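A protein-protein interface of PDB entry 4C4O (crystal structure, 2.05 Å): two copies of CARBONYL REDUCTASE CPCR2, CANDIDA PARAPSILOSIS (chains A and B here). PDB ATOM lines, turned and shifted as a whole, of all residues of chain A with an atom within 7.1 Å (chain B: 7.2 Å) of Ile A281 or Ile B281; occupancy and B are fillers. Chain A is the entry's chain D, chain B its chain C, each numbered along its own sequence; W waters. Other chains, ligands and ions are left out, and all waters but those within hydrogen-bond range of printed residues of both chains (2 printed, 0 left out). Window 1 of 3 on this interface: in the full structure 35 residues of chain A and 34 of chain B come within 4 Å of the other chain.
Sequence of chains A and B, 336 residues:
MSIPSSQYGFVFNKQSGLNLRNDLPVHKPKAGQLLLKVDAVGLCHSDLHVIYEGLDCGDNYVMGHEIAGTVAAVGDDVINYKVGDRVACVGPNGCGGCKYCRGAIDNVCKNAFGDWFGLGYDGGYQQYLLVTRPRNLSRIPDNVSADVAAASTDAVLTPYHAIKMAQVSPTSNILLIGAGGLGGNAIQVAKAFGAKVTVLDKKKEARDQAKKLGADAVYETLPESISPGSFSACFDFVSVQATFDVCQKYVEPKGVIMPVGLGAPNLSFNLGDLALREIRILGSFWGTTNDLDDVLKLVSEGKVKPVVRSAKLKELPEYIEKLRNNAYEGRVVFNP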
ATOM      1  N   PHE A 244      -8.225 -36.991  -5.636  1.00  0.00           N
ATOM      2  CA  PHE A 244      -8.887 -35.735  -5.968  1.00  0.00           C
ATOM      3  C   PHE A 244      -8.475 -35.236  -7.339  1.00  0.00           C
ATOM      4  O   PHE A 244      -9.320 -34.816  -8.131  1.00  0.00           O
ATOM      5  CB  PHE A 244      -8.757 -34.666  -4.825  1.00  0.00           C
ATOM      6  CG  PHE A 244      -9.587 -33.427  -5.081  1.00  0.00           C
ATOM      7  CD1 PHE A 244      -9.118 -32.456  -5.922  1.00  0.00           C
ATOM      8  CD2 PHE A 244     -10.902 -33.335  -4.622  1.00  0.00           C
ATOM      9  CE1 PHE A 244      -9.926 -31.349  -6.228  1.00  0.00           C
ATOM     10  CE2 PHE A 244     -11.711 -32.239  -4.928  1.00  0.00           C
ATOM     11  CZ  PHE A 244     -11.217 -31.225  -5.704  1.00  0.00           C
ATOM     12  N   GLN A 248     -10.683 -34.349 -10.644  1.00  0.00           N
ATOM     13  CA  GLN A 248     -10.693 -33.068 -11.278  1.00  0.00           C
ATOM     14  C   GLN A 248     -10.295 -33.135 -12.746  1.00  0.00           C
ATOM     15  O   GLN A 248     -10.802 -32.403 -13.550  1.00  0.00           O
ATOM     16  CB  GLN A 248      -9.877 -31.997 -10.498  1.00  0.00           C
ATOM     17  CG  GLN A 248     -10.058 -30.656 -11.168  1.00  0.00           C
ATOM     18  CD  GLN A 248      -9.688 -29.458 -10.352  1.00  0.00           C
ATOM     19  OE1 GLN A 248      -9.000 -29.539  -9.329  1.00  0.00           O
ATOM     20  NE2 GLN A 248     -10.115 -28.288 -10.841  1.00  0.00           N
ATOM     21  N   GLY A 255     -19.723 -30.571 -14.114  1.00  0.00           N
ATOM     22  CA  GLY A 255     -19.906 -31.805 -13.397  1.00  0.00           C
ATOM     23  C   GLY A 255     -19.592 -31.631 -11.935  1.00  0.00           C
ATOM     24  O   GLY A 255     -19.233 -30.561 -11.482  1.00  0.00           O
ATOM     25  N   VAL A 256     -19.768 -32.700 -11.184  1.00  0.00           N
ATOM     26  CA  VAL A 256     -19.606 -32.612  -9.762  1.00  0.00           C
ATOM     27  C   VAL A 256     -18.537 -33.592  -9.240  1.00  0.00           C
ATOM     28  O   VAL A 256     -18.473 -34.754  -9.672  1.00  0.00           O
ATOM     29  CB  VAL A 256     -20.981 -32.825  -9.032  1.00  0.00           C
ATOM     30  CG1 VAL A 256     -21.604 -34.135  -9.399  1.00  0.00           C
ATOM     31  CG2 VAL A 256     -20.810 -32.775  -7.528  1.00  0.00           C
ATOM     32  N   ILE A 257     -17.773 -33.128  -8.260  1.00  0.00           N
ATOM     33  CA  ILE A 257     -16.812 -33.990  -7.487  1.00  0.00           C
ATOM     34  C   ILE A 257     -17.311 -34.088  -6.067  1.00  0.00           C
ATOM     35  O   ILE A 257     -17.688 -33.055  -5.449  1.00  0.00           O
ATOM     36  CB  ILE A 257     -15.425 -33.379  -7.440  1.00  0.00           C
ATOM     37  CG1 ILE A 257     -14.881 -33.241  -8.828  1.00  0.00           C
ATOM     38  CG2 ILE A 257     -14.522 -34.224  -6.553  1.00  0.00           C
ATOM     39  CD1 ILE A 257     -13.614 -32.384  -8.888  1.00  0.00           C
ATOM     40  N   MET A 258     -17.497 -35.296  -5.597  1.00  0.00           N
ATOM     41  CA  MET A 258     -18.020 -35.526  -4.263  1.00  0.00           C
ATOM     42  C   MET A 258     -16.922 -36.220  -3.439  1.00  0.00           C
ATOM     43  O   MET A 258     -16.716 -37.442  -3.544  1.00  0.00           O
ATOM     44  CB  MET A 258     -19.193 -36.456  -4.280  1.00  0.00           C
ATOM     45  CG  MET A 258     -20.209 -36.170  -5.339  1.00  0.00           C
ATOM     46  SD  MET A 258     -21.344 -34.916  -4.745  1.00  0.00           S
ATOM     47  CE  MET A 258     -22.084 -35.643  -3.328  1.00  0.00           C
ATOM     48  N   PRO A 259     -16.230 -35.462  -2.617  1.00  0.00           N
ATOM     49  CA  PRO A 259     -15.157 -36.071  -1.809  1.00  0.00           C
ATOM     50  C   PRO A 259     -15.755 -36.646  -0.540  1.00  0.00           C
ATOM     51  O   PRO A 259     -15.794 -35.993   0.493  1.00  0.00           O
ATOM     52  CB  PRO A 259     -14.251 -34.904  -1.503  1.00  0.00           C
ATOM     53  CG  PRO A 259     -15.125 -33.732  -1.502  1.00  0.00           C
ATOM     54  CD  PRO A 259     -16.308 -34.015  -2.413  1.00  0.00           C
ATOM     55  N   SER A 268      -6.588 -29.799  -2.217  1.00  0.00           N
ATOM     56  CA  SER A 268      -6.560 -28.623  -3.026  1.00  0.00           C
ATOM     57  C   SER A 268      -7.141 -28.866  -4.398  1.00  0.00           C
ATOM     58  O   SER A 268      -7.084 -29.977  -4.947  1.00  0.00           O
ATOM     59  CB  SER A 268      -5.146 -28.049  -3.051  1.00  0.00           C
ATOM     60  OG  SER A 268      -4.515 -28.327  -4.215  1.00  0.00           O
ATOM     61  N   PHE A 269      -7.694 -27.816  -4.974  1.00  0.00           N
ATOM     62  CA  PHE A 269      -8.181 -27.869  -6.345  1.00  0.00           C
ATOM     63  C   PHE A 269      -7.563 -26.821  -7.158  1.00  0.00           C
ATOM     64  O   PHE A 269      -7.125 -25.796  -6.623  1.00  0.00           O
ATOM     65  CB  PHE A 269      -9.726 -27.717  -6.317  1.00  0.00           C
ATOM     66  CG  PHE A 269     -10.227 -26.394  -5.760  1.00  0.00           C
ATOM     67  CD1 PHE A 269     -10.367 -25.292  -6.584  1.00  0.00           C
ATOM     68  CD2 PHE A 269     -10.619 -26.282  -4.470  1.00  0.00           C
ATOM     69  CE1 PHE A 269     -10.897 -24.108  -6.101  1.00  0.00           C
ATOM     70  CE2 PHE A 269     -11.118 -25.102  -3.950  1.00  0.00           C
ATOM     71  CZ  PHE A 269     -11.225 -24.001  -4.762  1.00  0.00           C
ATOM     72  N   LEU A 274     -11.447 -25.151 -12.122  1.00  0.00           N
ATOM     73  CA  LEU A 274     -12.743 -25.188 -11.465  1.00  0.00           C
ATOM     74  C   LEU A 274     -13.667 -24.044 -11.949  1.00  0.00           C
ATOM     75  O   LEU A 274     -14.818 -24.275 -12.288  1.00  0.00           O
ATOM     76  CB  LEU A 274     -12.577 -25.175  -9.961  1.00  0.00           C
ATOM     77  CG  LEU A 274     -13.895 -25.105  -9.209  1.00  0.00           C
ATOM     78  CD1 LEU A 274     -14.005 -26.174  -8.215  1.00  0.00           C
ATOM     79  CD2 LEU A 274     -14.107 -23.754  -8.531  1.00  0.00           C
ATOM     80  N   GLU A 278     -16.573 -24.698 -14.640  1.00  0.00           N
ATOM     81  CA  GLU A 278     -17.706 -24.624 -13.670  1.00  0.00           C
ATOM     82  C   GLU A 278     -17.920 -25.901 -12.933  1.00  0.00           C
ATOM     83  O   GLU A 278     -19.028 -26.407 -12.829  1.00  0.00           O
ATOM     84  CB  GLU A 278     -18.992 -24.119 -14.350  1.00  0.00           C
ATOM     85  CG  GLU A 278     -18.815 -22.728 -14.928  1.00  0.00           C
ATOM     86  CD  GLU A 278     -20.151 -21.991 -15.152  1.00  0.00           C
ATOM     87  OE1 GLU A 278     -21.143 -22.669 -15.443  1.00  0.00           O
ATOM     88  OE2 GLU A 278     -20.170 -20.750 -15.098  1.00  0.00           O
ATOM     89  N   ILE A 279     -16.824 -26.417 -12.389  1.00  0.00           N
ATOM     90  CA  ILE A 279     -16.890 -27.639 -11.604  1.00  0.00           C
ATOM     91  C   ILE A 279     -17.472 -27.297 -10.235  1.00  0.00           C
ATOM     92  O   ILE A 279     -17.260 -26.230  -9.734  1.00  0.00           O
ATOM     93  CB  ILE A 279     -15.472 -28.271 -11.432  1.00  0.00           C
ATOM     94  CG1 ILE A 279     -14.797 -28.447 -12.791  1.00  0.00           C
ATOM     95  CG2 ILE A 279     -15.540 -29.609 -10.730  1.00  0.00           C
ATOM     96  CD1 ILE A 279     -15.616 -29.186 -13.802  1.00  0.00           C
ATOM     97  N   ARG A 280     -18.192 -28.240  -9.665  1.00  0.00           N
ATOM     98  CA  ARG A 280     -18.778 -28.105  -8.377  1.00  0.00           C
ATOM     99  C   ARG A 280     -18.210 -29.158  -7.483  1.00  0.00           C
ATOM    100  O   ARG A 280     -18.086 -30.318  -7.885  1.00  0.00           O
ATOM    101  CB  ARG A 280     -20.284 -28.367  -8.489  1.00  0.00           C
ATOM    102  CG  ARG A 280     -20.936 -27.419  -9.486  1.00  0.00           C
ATOM    103  CD  ARG A 280     -22.401 -27.743  -9.656  1.00  0.00           C
ATOM    104  NE  ARG A 280     -22.543 -28.828 -10.615  1.00  0.00           N
ATOM    105  CZ  ARG A 280     -23.328 -29.902 -10.486  1.00  0.00           C
ATOM    106  NH1 ARG A 280     -24.120 -30.053  -9.413  1.00  0.00           N
ATOM    107  NH2 ARG A 280     -23.368 -30.797 -11.486  1.00  0.00           N
ATOM    108  N   ILE A 281     -17.938 -28.794  -6.239  1.00  0.00           N
ATOM    109  CA  ILE A 281     -17.482 -29.737  -5.240  1.00  0.00           C
ATOM    110  C   ILE A 281     -18.499 -29.667  -4.171  1.00  0.00           C
ATOM    111  O   ILE A 281     -18.697 -28.593  -3.587  1.00  0.00           O
ATOM    112  CB  ILE A 281     -16.095 -29.289  -4.664  1.00  0.00           C
ATOM    113  CG1 ILE A 281     -15.032 -29.236  -5.762  1.00  0.00           C
ATOM    114  CG2 ILE A 281     -15.652 -30.256  -3.604  1.00  0.00           C
ATOM    115  CD1 ILE A 281     -13.750 -28.561  -5.325  1.00  0.00           C
ATOM    116  N   LEU A 282     -19.133 -30.783  -3.846  1.00  0.00           N
ATOM    117  CA  LEU A 282     -20.182 -30.785  -2.862  1.00  0.00           C
ATOM    118  C   LEU A 282     -19.845 -31.687  -1.679  1.00  0.00           C
ATOM    119  O   LEU A 282     -19.606 -32.900  -1.863  1.00  0.00           O
ATOM    120  CB  LEU A 282     -21.485 -31.369  -3.521  1.00  0.00           C
ATOM    121  CG  LEU A 282     -21.959 -30.718  -4.784  1.00  0.00           C
ATOM    122  CD1 LEU A 282     -23.349 -31.282  -5.175  1.00  0.00           C
ATOM    123  CD2 LEU A 282     -22.070 -29.232  -4.657  1.00  0.00           C
ATOM    124  N   GLY A 283     -19.826 -31.129  -0.484  1.00  0.00           N
ATOM    125  CA  GLY A 283     -19.683 -31.943   0.710  1.00  0.00           C
ATOM    126  C   GLY A 283     -20.954 -32.682   1.030  1.00  0.00           C
ATOM    127  O   GLY A 283     -22.065 -32.185   0.795  1.00  0.00           O
ATOM    128  N   PHE B 244     -10.028 -17.435   0.879  1.00  0.00           N
ATOM    129  CA  PHE B 244     -10.758 -18.717   0.855  1.00  0.00           C
ATOM    130  C   PHE B 244     -11.013 -19.218   2.250  1.00  0.00           C
ATOM    131  O   PHE B 244     -12.150 -19.632   2.578  1.00  0.00           O
ATOM    132  CB  PHE B 244     -10.101 -19.764  -0.080  1.00  0.00           C
ATOM    133  CG  PHE B 244     -10.912 -21.017  -0.221  1.00  0.00           C
ATOM    134  CD1 PHE B 244     -10.855 -22.003   0.755  1.00  0.00           C
ATOM    135  CD2 PHE B 244     -11.887 -21.119  -1.224  1.00  0.00           C
ATOM    136  CE1 PHE B 244     -11.676 -23.109   0.679  1.00  0.00           C
ATOM    137  CE2 PHE B 244     -12.664 -22.241  -1.343  1.00  0.00           C
ATOM    138  CZ  PHE B 244     -12.621 -23.208  -0.349  1.00  0.00           C
ATOM    139  N   GLN B 248     -14.539 -20.145   4.079  1.00  0.00           N
ATOM    140  CA  GLN B 248     -14.807 -21.447   4.701  1.00  0.00           C
ATOM    141  C   GLN B 248     -15.119 -21.365   6.174  1.00  0.00           C
ATOM    142  O   GLN B 248     -15.943 -22.093   6.672  1.00  0.00           O
ATOM    143  CB  GLN B 248     -13.698 -22.489   4.429  1.00  0.00           C
ATOM    144  CG  GLN B 248     -14.141 -23.815   4.944  1.00  0.00           C
ATOM    145  CD  GLN B 248     -13.352 -25.022   4.452  1.00  0.00           C
ATOM    146  OE1 GLN B 248     -12.271 -24.916   3.886  1.00  0.00           O
ATOM    147  NE2 GLN B 248     -13.942 -26.201   4.675  1.00  0.00           N
ATOM    148  N   GLY B 255     -24.045 -24.087   2.975  1.00  0.00           N
ATOM    149  CA  GLY B 255     -23.885 -22.861   2.266  1.00  0.00           C
ATOM    150  C   GLY B 255     -22.936 -23.015   1.124  1.00  0.00           C
ATOM    151  O   GLY B 255     -22.381 -24.108   0.897  1.00  0.00           O
ATOM    152  N   VAL B 256     -22.735 -21.945   0.385  1.00  0.00           N
ATOM    153  CA  VAL B 256     -21.936 -22.037  -0.830  1.00  0.00           C
ATOM    154  C   VAL B 256     -20.783 -21.027  -0.808  1.00  0.00           C
ATOM    155  O   VAL B 256     -20.923 -19.852  -0.372  1.00  0.00           O
ATOM    156  CB  VAL B 256     -22.798 -21.870  -2.099  1.00  0.00           C
ATOM    157  CG1 VAL B 256     -23.522 -20.535  -2.076  1.00  0.00           C
ATOM    158  CG2 VAL B 256     -21.948 -21.899  -3.338  1.00  0.00           C
ATOM    159  N   ILE B 257     -19.630 -21.480  -1.274  1.00  0.00           N
ATOM    160  CA  ILE B 257     -18.482 -20.609  -1.514  1.00  0.00           C
ATOM    161  C   ILE B 257     -18.303 -20.492  -3.004  1.00  0.00           C
ATOM    162  O   ILE B 257     -18.222 -21.526  -3.705  1.00  0.00           O
ATOM    163  CB  ILE B 257     -17.200 -21.194  -0.883  1.00  0.00           C
ATOM    164  CG1 ILE B 257     -17.353 -21.330   0.599  1.00  0.00           C
ATOM    165  CG2 ILE B 257     -16.008 -20.319  -1.236  1.00  0.00           C
ATOM    166  CD1 ILE B 257     -16.237 -22.159   1.263  1.00  0.00           C
ATOM    167  N   MET B 258     -18.201 -19.278  -3.511  1.00  0.00           N
ATOM    168  CA  MET B 258     -18.024 -19.019  -4.923  1.00  0.00           C
ATOM    169  C   MET B 258     -16.675 -18.300  -5.157  1.00  0.00           C
ATOM    170  O   MET B 258     -16.547 -17.080  -4.964  1.00  0.00           O
ATOM    171  CB  MET B 258     -19.068 -18.094  -5.439  1.00  0.00           C
ATOM    172  CG  MET B 258     -20.471 -18.422  -4.995  1.00  0.00           C
ATOM    173  SD  MET B 258     -21.126 -19.723  -6.034  1.00  0.00           S
ATOM    174  CE  MET B 258     -21.154 -18.985  -7.642  1.00  0.00           C
ATOM    175  N   PRO B 259     -15.663 -19.051  -5.543  1.00  0.00           N
ATOM    176  CA  PRO B 259     -14.345 -18.393  -5.768  1.00  0.00           C
ATOM    177  C   PRO B 259     -14.297 -17.816  -7.176  1.00  0.00           C
ATOM    178  O   PRO B 259     -13.846 -18.481  -8.105  1.00  0.00           O
ATOM    179  CB  PRO B 259     -13.352 -19.559  -5.604  1.00  0.00           C
ATOM    180  CG  PRO B 259     -14.119 -20.754  -6.004  1.00  0.00           C
ATOM    181  CD  PRO B 259     -15.596 -20.506  -5.738  1.00  0.00           C
ATOM    182  N   SER B 268      -6.859 -24.589  -1.268  1.00  0.00           N
ATOM    183  CA  SER B 268      -7.186 -25.760  -0.529  1.00  0.00           C
ATOM    184  C   SER B 268      -8.290 -25.533   0.457  1.00  0.00           C
ATOM    185  O   SER B 268      -8.545 -24.405   0.909  1.00  0.00           O
ATOM    186  CB  SER B 268      -5.898 -26.324   0.114  1.00  0.00           C
ATOM    187  OG  SER B 268      -5.905 -26.029   1.449  1.00  0.00           O
ATOM    188  N   PHE B 269      -9.009 -26.602   0.741  1.00  0.00           N
ATOM    189  CA  PHE B 269     -10.132 -26.558   1.674  1.00  0.00           C
ATOM    190  C   PHE B 269      -9.917 -27.593   2.678  1.00  0.00           C
ATOM    191  O   PHE B 269      -9.342 -28.653   2.391  1.00  0.00           O
ATOM    192  CB  PHE B 269     -11.498 -26.757   0.932  1.00  0.00           C
ATOM    193  CG  PHE B 269     -11.670 -28.076   0.222  1.00  0.00           C
ATOM    194  CD1 PHE B 269     -12.203 -29.153   0.843  1.00  0.00           C
ATOM    195  CD2 PHE B 269     -11.376 -28.173  -1.131  1.00  0.00           C
ATOM    196  CE1 PHE B 269     -12.384 -30.356   0.185  1.00  0.00           C
ATOM    197  CE2 PHE B 269     -11.521 -29.362  -1.797  1.00  0.00           C
ATOM    198  CZ  PHE B 269     -12.056 -30.461  -1.135  1.00  0.00           C
ATOM    199  N   LEU B 274     -15.697 -29.333   5.210  1.00  0.00           N
ATOM    200  CA  LEU B 274     -16.552 -29.345   4.021  1.00  0.00           C
ATOM    201  C   LEU B 274     -17.568 -30.515   4.022  1.00  0.00           C
ATOM    202  O   LEU B 274     -18.743 -30.320   3.725  1.00  0.00           O
ATOM    203  CB  LEU B 274     -15.693 -29.354   2.766  1.00  0.00           C
ATOM    204  CG  LEU B 274     -16.495 -29.431   1.475  1.00  0.00           C
ATOM    205  CD1 LEU B 274     -16.097 -28.360   0.512  1.00  0.00           C
ATOM    206  CD2 LEU B 274     -16.345 -30.780   0.795  1.00  0.00           C
ATOM    207  N   GLU B 278     -21.408 -29.946   4.978  1.00  0.00           N
ATOM    208  CA  GLU B 278     -21.940 -30.045   3.607  1.00  0.00           C
ATOM    209  C   GLU B 278     -21.806 -28.752   2.819  1.00  0.00           C
ATOM    210  O   GLU B 278     -22.770 -28.236   2.238  1.00  0.00           O
ATOM    211  CB  GLU B 278     -23.397 -30.559   3.607  1.00  0.00           C
ATOM    212  CG  GLU B 278     -23.525 -31.935   4.182  1.00  0.00           C
ATOM    213  CD  GLU B 278     -24.796 -32.658   3.789  1.00  0.00           C
ATOM    214  OE1 GLU B 278     -25.813 -31.988   3.564  1.00  0.00           O
ATOM    215  OE2 GLU B 278     -24.818 -33.908   3.753  1.00  0.00           O
ATOM    216  N   ILE B 279     -20.601 -28.204   2.814  1.00  0.00           N
ATOM    217  CA  ILE B 279     -20.352 -26.957   2.138  1.00  0.00           C
ATOM    218  C   ILE B 279     -20.216 -27.278   0.667  1.00  0.00           C
ATOM    219  O   ILE B 279     -19.739 -28.363   0.303  1.00  0.00           O
ATOM    220  CB  ILE B 279     -19.021 -26.298   2.641  1.00  0.00           C
ATOM    221  CG1 ILE B 279     -19.025 -26.144   4.160  1.00  0.00           C
ATOM    222  CG2 ILE B 279     -18.775 -24.994   1.978  1.00  0.00           C
ATOM    223  CD1 ILE B 279     -20.263 -25.390   4.656  1.00  0.00           C
ATOM    224  N   ARG B 280     -20.575 -26.315  -0.174  1.00  0.00           N
ATOM    225  CA  ARG B 280     -20.490 -26.466  -1.596  1.00  0.00           C
ATOM    226  C   ARG B 280     -19.572 -25.399  -2.154  1.00  0.00           C
ATOM    227  O   ARG B 280     -19.643 -24.278  -1.710  1.00  0.00           O
ATOM    228  CB  ARG B 280     -21.905 -26.258  -2.187  1.00  0.00           C
ATOM    229  CG  ARG B 280     -22.918 -27.236  -1.624  1.00  0.00           C
ATOM    230  CD  ARG B 280     -24.286 -26.952  -2.176  1.00  0.00           C
ATOM    231  NE  ARG B 280     -24.895 -25.866  -1.401  1.00  0.00           N
ATOM    232  CZ  ARG B 280     -25.516 -24.796  -1.898  1.00  0.00           C
ATOM    233  NH1 ARG B 280     -25.707 -24.669  -3.219  1.00  0.00           N
ATOM    234  NH2 ARG B 280     -25.974 -23.846  -1.056  1.00  0.00           N
ATOM    235  N   ILE B 281     -18.707 -25.761  -3.099  1.00  0.00           N
ATOM    236  CA  ILE B 281     -17.827 -24.816  -3.757  1.00  0.00           C
ATOM    237  C   ILE B 281     -18.233 -24.898  -5.220  1.00  0.00           C
ATOM    238  O   ILE B 281     -18.135 -25.952  -5.832  1.00  0.00           O
ATOM    239  CB  ILE B 281     -16.337 -25.234  -3.629  1.00  0.00           C
ATOM    240  CG1 ILE B 281     -15.907 -25.289  -2.160  1.00  0.00           C
ATOM    241  CG2 ILE B 281     -15.473 -24.244  -4.343  1.00  0.00           C
ATOM    242  CD1 ILE B 281     -14.560 -25.954  -1.938  1.00  0.00           C
ATOM    243  N   LEU B 282     -18.656 -23.805  -5.792  1.00  0.00           N
ATOM    244  CA  LEU B 282     -19.153 -23.786  -7.153  1.00  0.00           C
ATOM    245  C   LEU B 282     -18.323 -22.880  -8.026  1.00  0.00           C
ATOM    246  O   LEU B 282     -18.240 -21.661  -7.780  1.00  0.00           O
ATOM    247  CB  LEU B 282     -20.609 -23.279  -7.194  1.00  0.00           C
ATOM    248  CG  LEU B 282     -21.608 -23.958  -6.277  1.00  0.00           C
ATOM    249  CD1 LEU B 282     -23.016 -23.418  -6.573  1.00  0.00           C
ATOM    250  CD2 LEU B 282     -21.638 -25.457  -6.418  1.00  0.00           C
ATOM    251  N   GLY B 283     -17.764 -23.433  -9.102  1.00  0.00           N
ATOM    252  CA  GLY B 283     -17.103 -22.621 -10.091  1.00  0.00           C
ATOM    253  C   GLY B 283     -18.089 -21.883 -10.987  1.00  0.00           C
ATOM    254  O   GLY B 283     -19.173 -22.396 -11.281  1.00  0.00           O
HETATM  255  O   HOH W   1     -23.315 -30.093  -0.163  1.00  0.00           O
HETATM  256  O   HOH W   2     -20.808 -24.439 -10.958  1.00  0.00           O
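The backbone carbonyl oxygen of Ile B279 is in hydrogen-bond range of the backbone NH of Gly A283, at 2.9 Å.
The backbone carbonyl oxygen (O) of Ile A281 is in hydrogen-bond range of the backbone NH (N) of Ile B281 (2.9 Å).
The backbone NH (N) of Gly B283 sits at hydrogen-bond distance from the backbone carbonyl oxygen (O) of Ile A279 (2.9 Å).
The backbone carbonyl oxygen of Gly B255 lies within hydrogen-bond range of the backbone NH of Arg B280.
The backbone NH of Ile B257 sits at hydrogen-bond distance from the backbone carbonyl oxygen of Arg B280 (2.8 Å).
The backbone carbonyl oxygen (O) of Leu B274 is in hydrogen-bond range of the backbone NH (N) of Ile B279, at 3.0 Å.
O of Gly A255 is in hydrogen-bond range of N of Arg A280 (3.1 Å).
The backbone carbonyl oxygen (O) of Arg A280 sits at hydrogen-bond distance from the backbone NH (N) of Ile A257 (2.9 Å).
The backbone carbonyl oxygen (O) of Ile A257 sits at hydrogen-bond distance from the backbone NH (N) of Leu A282 (3.1 Å).
Leu B274 touches Pro A259.
Phe B269 touches Phe A269 (CD2 to CD2, 3.9 Å).
Gly B283 touches Glu A278 (O to CB, 3.5 Å).
Leu B282 touches Ile A279.
Arg A280 touches Ile B281.
Arg A280 touches Leu B282 (CG to CD2, 3.7 Å).
O of Ile A281 touches CA of Arg B280 (3.4 Å).
Ile B279 touches Leu A282.
CD2 of Leu A282 touches CG of Arg B280, at 3.7 Å.
CB of Glu B278 touches O of Gly A283, at 3.5 Å.
Ile A281 touches two residues of chain B.
Printed residues of chain A within 4 Å of Ile B281: Arg A280 (3.4 Å) and Ile A281 (2.9 Å).
Of the printed residues of chain A, Ile B279 touches Leu A282 (3.9 Å) and Gly A283 (2.9 Å).
Of the printed residues of chain A, Phe B269 touches Phe A269 (3.9 Å).
Of the printed residues of chain B, Arg A280 touches Ile B281 (3.4 Å) and Leu B282 (3.7 Å).
Gln B248 touches none of the printed residues of chain A.
Of the 16 printed residues of chain B, 10 touch a printed residue of chain A.
Printed residues of chain B that touch a printed residue of chain A: Pro B259, Ser B268, Phe B269, Leu B274, Glu B278, Ile B279, Arg B280, Ile B281, Leu B282 and Gly B283.
Hydrophobic or aromatic side chains of chain B that line the printed part of chain A: Pro B259, Phe B269, Leu B274 and Leu B282.
Of the 16 printed residues of chain A, 10 touch a printed residue of chain B.
Printed residues of chain A that touch a printed residue of chain B: Pro A259, Ser A268, Phe A269, Leu A274, Glu A278, Ile A279, Arg A280, Ile A281, Leu A282 and Gly A283.
Hydrophobic or aromatic side chains of chain A within 4 Å of the printed part of chain B: Pro A259, Phe A269, Leu A274 and Leu A282.
Among the printed residues, no Asp or Glu carboxylate lies within 4 Å of a Lys or Arg side-chain nitrogen of the other chain.
Pro A259 touches Leu B274, and with the chains exchanged Leu A274 touches Pro B259.
Phe A269 touches its own counterpart, Phe B269.
Ile A279 touches Leu B282, and with the chains exchanged Leu A282 touches Ile B279.
Ile B281 touches its own counterpart, Ile A281.
16 positions are printed for both chains.
Of the 17 pairs that touch across the chains among the printed residues, 17 have their exchanged pair printed and touching as well.
Water W1 bridges the backbone carbonyl oxygen of Gly A283 (2.6 Å) and the backbone carbonyl oxygen of Glu B278 (3.1 Å).
Water W2 lies within hydrogen-bond range of the backbone carbonyl oxygen of Gly B283 and the backbone carbonyl oxygen of Glu A278.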
